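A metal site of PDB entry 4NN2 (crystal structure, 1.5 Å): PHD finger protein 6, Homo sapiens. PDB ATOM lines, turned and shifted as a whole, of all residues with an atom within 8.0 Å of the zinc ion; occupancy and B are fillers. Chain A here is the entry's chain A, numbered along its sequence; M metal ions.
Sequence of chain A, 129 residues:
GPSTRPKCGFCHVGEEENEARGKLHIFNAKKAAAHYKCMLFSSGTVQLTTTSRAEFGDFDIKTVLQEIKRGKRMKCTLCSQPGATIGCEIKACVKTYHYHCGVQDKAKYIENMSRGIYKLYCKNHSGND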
ATOM      1  N   PHE A  10      -3.763  11.972  -9.969  1.00  0.00           N
ATOM      2  CA  PHE A  10      -2.964  12.671 -10.963  1.00  0.00           C
ATOM      3  C   PHE A  10      -1.543  12.961 -10.484  1.00  0.00           C
ATOM      4  O   PHE A  10      -0.560  12.534 -11.118  1.00  0.00           O
ATOM      5  CB  PHE A  10      -3.683  13.974 -11.370  1.00  0.00           C
ATOM      6  CG  PHE A  10      -5.035  13.744 -11.988  1.00  0.00           C
ATOM      7  CD1 PHE A  10      -5.145  13.152 -13.233  1.00  0.00           C
ATOM      8  CD2 PHE A  10      -6.197  14.081 -11.306  1.00  0.00           C
ATOM      9  CE1 PHE A  10      -6.388  12.924 -13.810  1.00  0.00           C
ATOM     10  CE2 PHE A  10      -7.439  13.850 -11.873  1.00  0.00           C
ATOM     11  CZ  PHE A  10      -7.540  13.284 -13.132  1.00  0.00           C
ATOM     12  N   CYS A  11      -1.415  13.693  -9.378  1.00  0.00           N
ATOM     13  CA  CYS A  11      -0.118  14.158  -8.903  1.00  0.00           C
ATOM     14  C   CYS A  11       0.466  13.325  -7.750  1.00  0.00           C
ATOM     15  O   CYS A  11       1.609  13.559  -7.358  1.00  0.00           O
ATOM     16  CB  CYS A  11      -0.154  15.635  -8.508  1.00  0.00           C
ATOM     17  SG  CYS A  11      -1.060  15.970  -6.978  1.00  0.00           S
ATOM     18  N   HIS A  12      -0.305  12.379  -7.226  1.00  0.00           N
ATOM     19  CA  HIS A  12       0.204  11.378  -6.263  1.00  0.00           C
ATOM     20  C   HIS A  12       0.495  11.937  -4.882  1.00  0.00           C
ATOM     21  O   HIS A  12       1.255  11.338  -4.122  1.00  0.00           O
ATOM     22  CB  HIS A  12       1.454  10.679  -6.824  1.00  0.00           C
ATOM     23  CG  HIS A  12       1.309  10.301  -8.250  1.00  0.00           C
ATOM     24  ND1 HIS A  12       0.362   9.410  -8.684  1.00  0.00           N
ATOM     25  CD2 HIS A  12       1.944  10.746  -9.353  1.00  0.00           C
ATOM     26  CE1 HIS A  12       0.431   9.297  -9.997  1.00  0.00           C
ATOM     27  NE2 HIS A  12       1.394  10.098 -10.426  1.00  0.00           N
ATOM     28  N   MET A  74       0.514   8.914 -19.282  1.00  0.00           N
ATOM     29  CA  MET A  74       0.954  10.286 -19.609  1.00  0.00           C
ATOM     30  C   MET A  74       2.087  10.815 -18.734  1.00  0.00           C
ATOM     31  O   MET A  74       1.851  11.272 -17.597  1.00  0.00           O
ATOM     32  CB  MET A  74      -0.230  11.242 -19.496  1.00  0.00           C
ATOM     33  CG  MET A  74      -1.477  10.825 -20.258  1.00  0.00           C
ATOM     34  SD  MET A  74      -1.254  10.641 -22.026  1.00  0.00           S
ATOM     35  CE  MET A  74      -0.508  12.202 -22.490  1.00  0.00           C
ATOM     36  N   LYS A  75       3.311  10.765 -19.246  1.00  0.00           N
ATOM     37  CA  LYS A  75       4.476  11.278 -18.541  1.00  0.00           C
ATOM     38  C   LYS A  75       4.551  12.798 -18.642  1.00  0.00           C
ATOM     39  O   LYS A  75       4.483  13.368 -19.732  1.00  0.00           O
ATOM     40  CB  LYS A  75       5.765  10.623 -19.070  1.00  0.00           C
ATOM     41  CG  LYS A  75       5.888   9.141 -18.743  1.00  0.00           C
ATOM     42  CD  LYS A  75       7.106   8.476 -19.357  1.00  0.00           C
ATOM     43  CE  LYS A  75       6.754   7.533 -20.509  1.00  0.00           C
ATOM     44  NZ  LYS A  75       7.809   6.505 -20.713  1.00  0.00           N
ATOM     45  N   CYS A  76       4.691  13.462 -17.512  1.00  0.00           N
ATOM     46  CA  CYS A  76       4.706  14.912 -17.435  1.00  0.00           C
ATOM     47  C   CYS A  76       5.836  15.520 -18.247  1.00  0.00           C
ATOM     48  O   CYS A  76       6.997  15.082 -18.169  1.00  0.00           O
ATOM     49  CB  CYS A  76       4.880  15.334 -15.977  1.00  0.00           C
ATOM     50  SG  CYS A  76       4.757  17.104 -15.638  1.00  0.00           S
ATOM     51  N   THR A  77       5.535  16.587 -18.976  1.00  0.00           N
ATOM     52  CA  THR A  77       6.552  17.330 -19.721  1.00  0.00           C
ATOM     53  C   THR A  77       7.707  17.800 -18.820  1.00  0.00           C
ATOM     54  O   THR A  77       8.869  17.810 -19.254  1.00  0.00           O
ATOM     55  CB  THR A  77       5.877  18.507 -20.429  1.00  0.00           C
ATOM     56  OG1 THR A  77       5.074  17.984 -21.489  1.00  0.00           O
ATOM     57  CG2 THR A  77       6.876  19.529 -20.986  1.00  0.00           C
ATOM     58  N   LEU A  78       7.392  18.178 -17.590  1.00  0.00           N
ATOM     59  CA  LEU A  78       8.396  18.691 -16.668  1.00  0.00           C
ATOM     60  C   LEU A  78       9.068  17.570 -15.861  1.00  0.00           C
ATOM     61  O   LEU A  78      10.283  17.396 -15.951  1.00  0.00           O
ATOM     62  CB  LEU A  78       7.787  19.739 -15.724  1.00  0.00           C
ATOM     63  CG  LEU A  78       8.806  20.444 -14.823  1.00  0.00           C
ATOM     64  CD1 LEU A  78       9.750  21.303 -15.661  1.00  0.00           C
ATOM     65  CD2 LEU A  78       8.102  21.274 -13.771  1.00  0.00           C
ATOM     66  N   CYS A  79       8.292  16.814 -15.079  1.00  0.00           N
ATOM     67  CA  CYS A  79       8.850  15.862 -14.102  1.00  0.00           C
ATOM     68  C   CYS A  79       8.966  14.412 -14.594  1.00  0.00           C
ATOM     69  O   CYS A  79       9.552  13.568 -13.899  1.00  0.00           O
ATOM     70  CB  CYS A  79       8.032  15.914 -12.783  1.00  0.00           C
ATOM     71  SG  CYS A  79       6.421  15.077 -12.860  1.00  0.00           S
ATOM     72  N   SER A  80       8.408  14.122 -15.768  1.00  0.00           N
ATOM     73  CA  SER A  80       8.462  12.810 -16.429  1.00  0.00           C
ATOM     74  C   SER A  80       7.684  11.693 -15.733  1.00  0.00           C
ATOM     75  O   SER A  80       7.733  10.542 -16.186  1.00  0.00           O
ATOM     76  CB  SER A  80       9.904  12.350 -16.668  1.00  0.00           C
ATOM     77  OG  SER A  80      10.626  13.275 -17.467  1.00  0.00           O
ATOM     78  N   GLN A  81       6.951  12.020 -14.661  1.00  0.00           N
ATOM     79  CA  GLN A  81       6.171  11.032 -13.941  1.00  0.00           C
ATOM     80  C   GLN A  81       4.744  10.966 -14.485  1.00  0.00           C
ATOM     81  O   GLN A  81       4.254  11.958 -15.026  1.00  0.00           O
ATOM     82  CB  GLN A  81       6.167  11.325 -12.445  1.00  0.00           C
ATOM     83  CG  GLN A  81       7.560  11.522 -11.855  1.00  0.00           C
ATOM     84  CD  GLN A  81       8.527  10.446 -12.310  1.00  0.00           C
ATOM     85  OE1 GLN A  81       9.485  10.709 -13.049  1.00  0.00           O
ATOM     86  NE2 GLN A  81       8.254   9.227 -11.922  1.00  0.00           N
ATOM     87  N   PRO A  82       4.081   9.800 -14.330  1.00  0.00           N
ATOM     88  CA  PRO A  82       2.726   9.644 -14.877  1.00  0.00           C
ATOM     89  C   PRO A  82       1.703  10.501 -14.149  1.00  0.00           C
ATOM     90  O   PRO A  82       2.005  11.039 -13.074  1.00  0.00           O
ATOM     91  CB  PRO A  82       2.420   8.159 -14.694  1.00  0.00           C
ATOM     92  CG  PRO A  82       3.438   7.629 -13.781  1.00  0.00           C
ATOM     93  CD  PRO A  82       4.607   8.547 -13.776  1.00  0.00           C
ATOM     94  N   GLY A  83       0.532  10.653 -14.748  1.00  0.00           N
ATOM     95  CA  GLY A  83      -0.589  11.406 -14.183  1.00  0.00           C
ATOM     96  C   GLY A  83      -0.758  12.787 -14.755  1.00  0.00           C
ATOM     97  O   GLY A  83      -1.638  13.529 -14.318  1.00  0.00           O
ATOM     98  N   ALA A  84       0.068  13.141 -15.728  1.00  0.00           N
ATOM     99  CA  ALA A  84       0.070  14.492 -16.329  1.00  0.00           C
ATOM    100  C   ALA A  84      -0.978  14.610 -17.446  1.00  0.00           C
ATOM    101  O   ALA A  84      -0.659  14.447 -18.628  1.00  0.00           O
ATOM    102  CB  ALA A  84       1.465  14.805 -16.869  1.00  0.00           C
ATOM    103  N   THR A  96       2.158  18.302 -21.825  1.00  0.00           N
ATOM    104  CA  THR A  96       1.094  17.847 -20.920  1.00  0.00           C
ATOM    105  C   THR A  96       1.649  17.784 -19.509  1.00  0.00           C
ATOM    106  O   THR A  96       2.806  17.427 -19.306  1.00  0.00           O
ATOM    107  CB  THR A  96       0.517  16.503 -21.403  1.00  0.00           C
ATOM    108  OG1 THR A  96      -0.700  16.203 -20.705  1.00  0.00           O
ATOM    109  CG2 THR A  96       1.524  15.345 -21.279  1.00  0.00           C
ATOM    110  N   TYR A  97       0.825  18.154 -18.529  1.00  0.00           N
ATOM    111  CA  TYR A  97       1.351  18.494 -17.197  1.00  0.00           C
ATOM    112  C   TYR A  97       0.506  18.003 -16.022  1.00  0.00           C
ATOM    113  O   TYR A  97      -0.709  17.831 -16.149  1.00  0.00           O
ATOM    114  CB  TYR A  97       1.415  20.012 -17.060  1.00  0.00           C
ATOM    115  CG  TYR A  97       2.444  20.691 -17.956  1.00  0.00           C
ATOM    116  CD1 TYR A  97       3.781  20.734 -17.605  1.00  0.00           C
ATOM    117  CD2 TYR A  97       2.044  21.332 -19.109  1.00  0.00           C
ATOM    118  CE1 TYR A  97       4.720  21.388 -18.415  1.00  0.00           C
ATOM    119  CE2 TYR A  97       2.953  21.994 -19.917  1.00  0.00           C
ATOM    120  CZ  TYR A  97       4.291  22.018 -19.571  1.00  0.00           C
ATOM    121  OH  TYR A  97       5.189  22.693 -20.385  1.00  0.00           O
ATOM    122  N   HIS A  98       1.175  17.821 -14.892  1.00  0.00           N
ATOM    123  CA  HIS A  98       0.526  17.952 -13.583  1.00  0.00           C
ATOM    124  C   HIS A  98       0.260  19.438 -13.319  1.00  0.00           C
ATOM    125  O   HIS A  98       1.022  20.293 -13.775  1.00  0.00           O
ATOM    126  CB  HIS A  98       1.423  17.428 -12.472  1.00  0.00           C
ATOM    127  CG  HIS A  98       1.787  15.993 -12.608  1.00  0.00           C
ATOM    128  ND1 HIS A  98       3.069  15.584 -12.936  1.00  0.00           N
ATOM    129  CD2 HIS A  98       1.053  14.872 -12.472  1.00  0.00           C
ATOM    130  CE1 HIS A  98       3.100  14.258 -12.970  1.00  0.00           C
ATOM    131  NE2 HIS A  98       1.889  13.803 -12.697  1.00  0.00           N
ATOM    132  N   TYR A  99      -0.781  19.749 -12.562  1.00  0.00           N
ATOM    133  CA  TYR A  99      -1.125  21.146 -12.322  1.00  0.00           C
ATOM    134  C   TYR A  99       0.063  21.991 -11.849  1.00  0.00           C
ATOM    135  O   TYR A  99       0.393  23.014 -12.467  1.00  0.00           O
ATOM    136  CB  TYR A  99      -2.313  21.280 -11.343  1.00  0.00           C
ATOM    137  CG  TYR A  99      -2.538  22.712 -10.949  1.00  0.00           C
ATOM    138  CD1 TYR A  99      -3.115  23.610 -11.846  1.00  0.00           C
ATOM    139  CD2 TYR A  99      -2.125  23.189  -9.714  1.00  0.00           C
ATOM    140  CE1 TYR A  99      -3.288  24.945 -11.510  1.00  0.00           C
ATOM    141  CE2 TYR A  99      -2.278  24.514  -9.380  1.00  0.00           C
ATOM    142  CZ  TYR A  99      -2.864  25.379 -10.266  1.00  0.00           C
ATOM    143  OH  TYR A  99      -3.027  26.714  -9.929  1.00  0.00           O
ATOM    144  N   HIS A 100       0.708  21.574 -10.772  1.00  0.00           N
ATOM    145  CA  HIS A 100       1.828  22.355 -10.223  1.00  0.00           C
ATOM    146  C   HIS A 100       3.021  22.421 -11.170  1.00  0.00           C
ATOM    147  O   HIS A 100       3.738  23.423 -11.213  1.00  0.00           O
ATOM    148  CB  HIS A 100       2.253  21.850  -8.837  1.00  0.00           C
ATOM    149  CG  HIS A 100       2.924  20.515  -8.853  1.00  0.00           C
ATOM    150  ND1 HIS A 100       2.253  19.346  -9.113  1.00  0.00           N
ATOM    151  CD2 HIS A 100       4.212  20.169  -8.606  1.00  0.00           C
ATOM    152  CE1 HIS A 100       3.106  18.336  -9.053  1.00  0.00           C
ATOM    153  NE2 HIS A 100       4.294  18.814  -8.720  1.00  0.00           N
ATOM    154  N   CYS A 101       3.239  21.361 -11.950  1.00  0.00           N
ATOM    155  CA  CYS A 101       4.315  21.342 -12.940  1.00  0.00           C
ATOM    156  C   CYS A 101       4.067  22.342 -14.070  1.00  0.00           C
ATOM    157  O   CYS A 101       5.005  22.978 -14.543  1.00  0.00           O
ATOM    158  CB  CYS A 101       4.490  19.938 -13.482  1.00  0.00           C
ATOM    159  SG  CYS A 101       4.972  18.737 -12.199  1.00  0.00           S
ATOM    160  N   GLY A 102       2.815  22.478 -14.498  1.00  0.00           N
ATOM    161  CA  GLY A 102       2.457  23.490 -15.489  1.00  0.00           C
ATOM    162  C   GLY A 102       2.762  24.894 -15.021  1.00  0.00           C
ATOM    163  O   GLY A 102       3.276  25.710 -15.776  1.00  0.00           O
HETATM  164 ZN    ZN M   1       4.854  16.751 -13.341  1.00  0.00          ZN
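NE2 of His 98 sits close to O of Phe 10 (3.2 Å). The backbone carbonyl oxygen of Gln 81 lies within hydrogen-bond range of the backbone NH of Cys 76, 2.9 Å away. The backbone carbonyl oxygen of Pro 82 sits at hydrogen-bond distance from a ring nitrogen (NE2) of His 98 (2.8 Å). A ring nitrogen (NE2) of His 100 sits close to the side-chain sulfur of Cys 101 (3.5 Å). N of Leu 78 lies close to SG of Cys 76, at 3.5 Å. The backbone carbonyl oxygen (O) of Cys 79 lies close to the side-chain amide oxygen (OE1) of Gln 81, at 3.0 Å.
A ring nitrogen (ND1) of His 98 is bound to the zinc ion (2.2 Å). The zinc ion is bound by SG of Cys 101. SG of Cys 76 binds the zinc ion. The zinc ion is bound by SG of Cys 79, 2.3 Å away.
Four residues have an atom within 4 Å of the zinc ion: Cys 76, Cys 79, His 98 and Cys 101.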
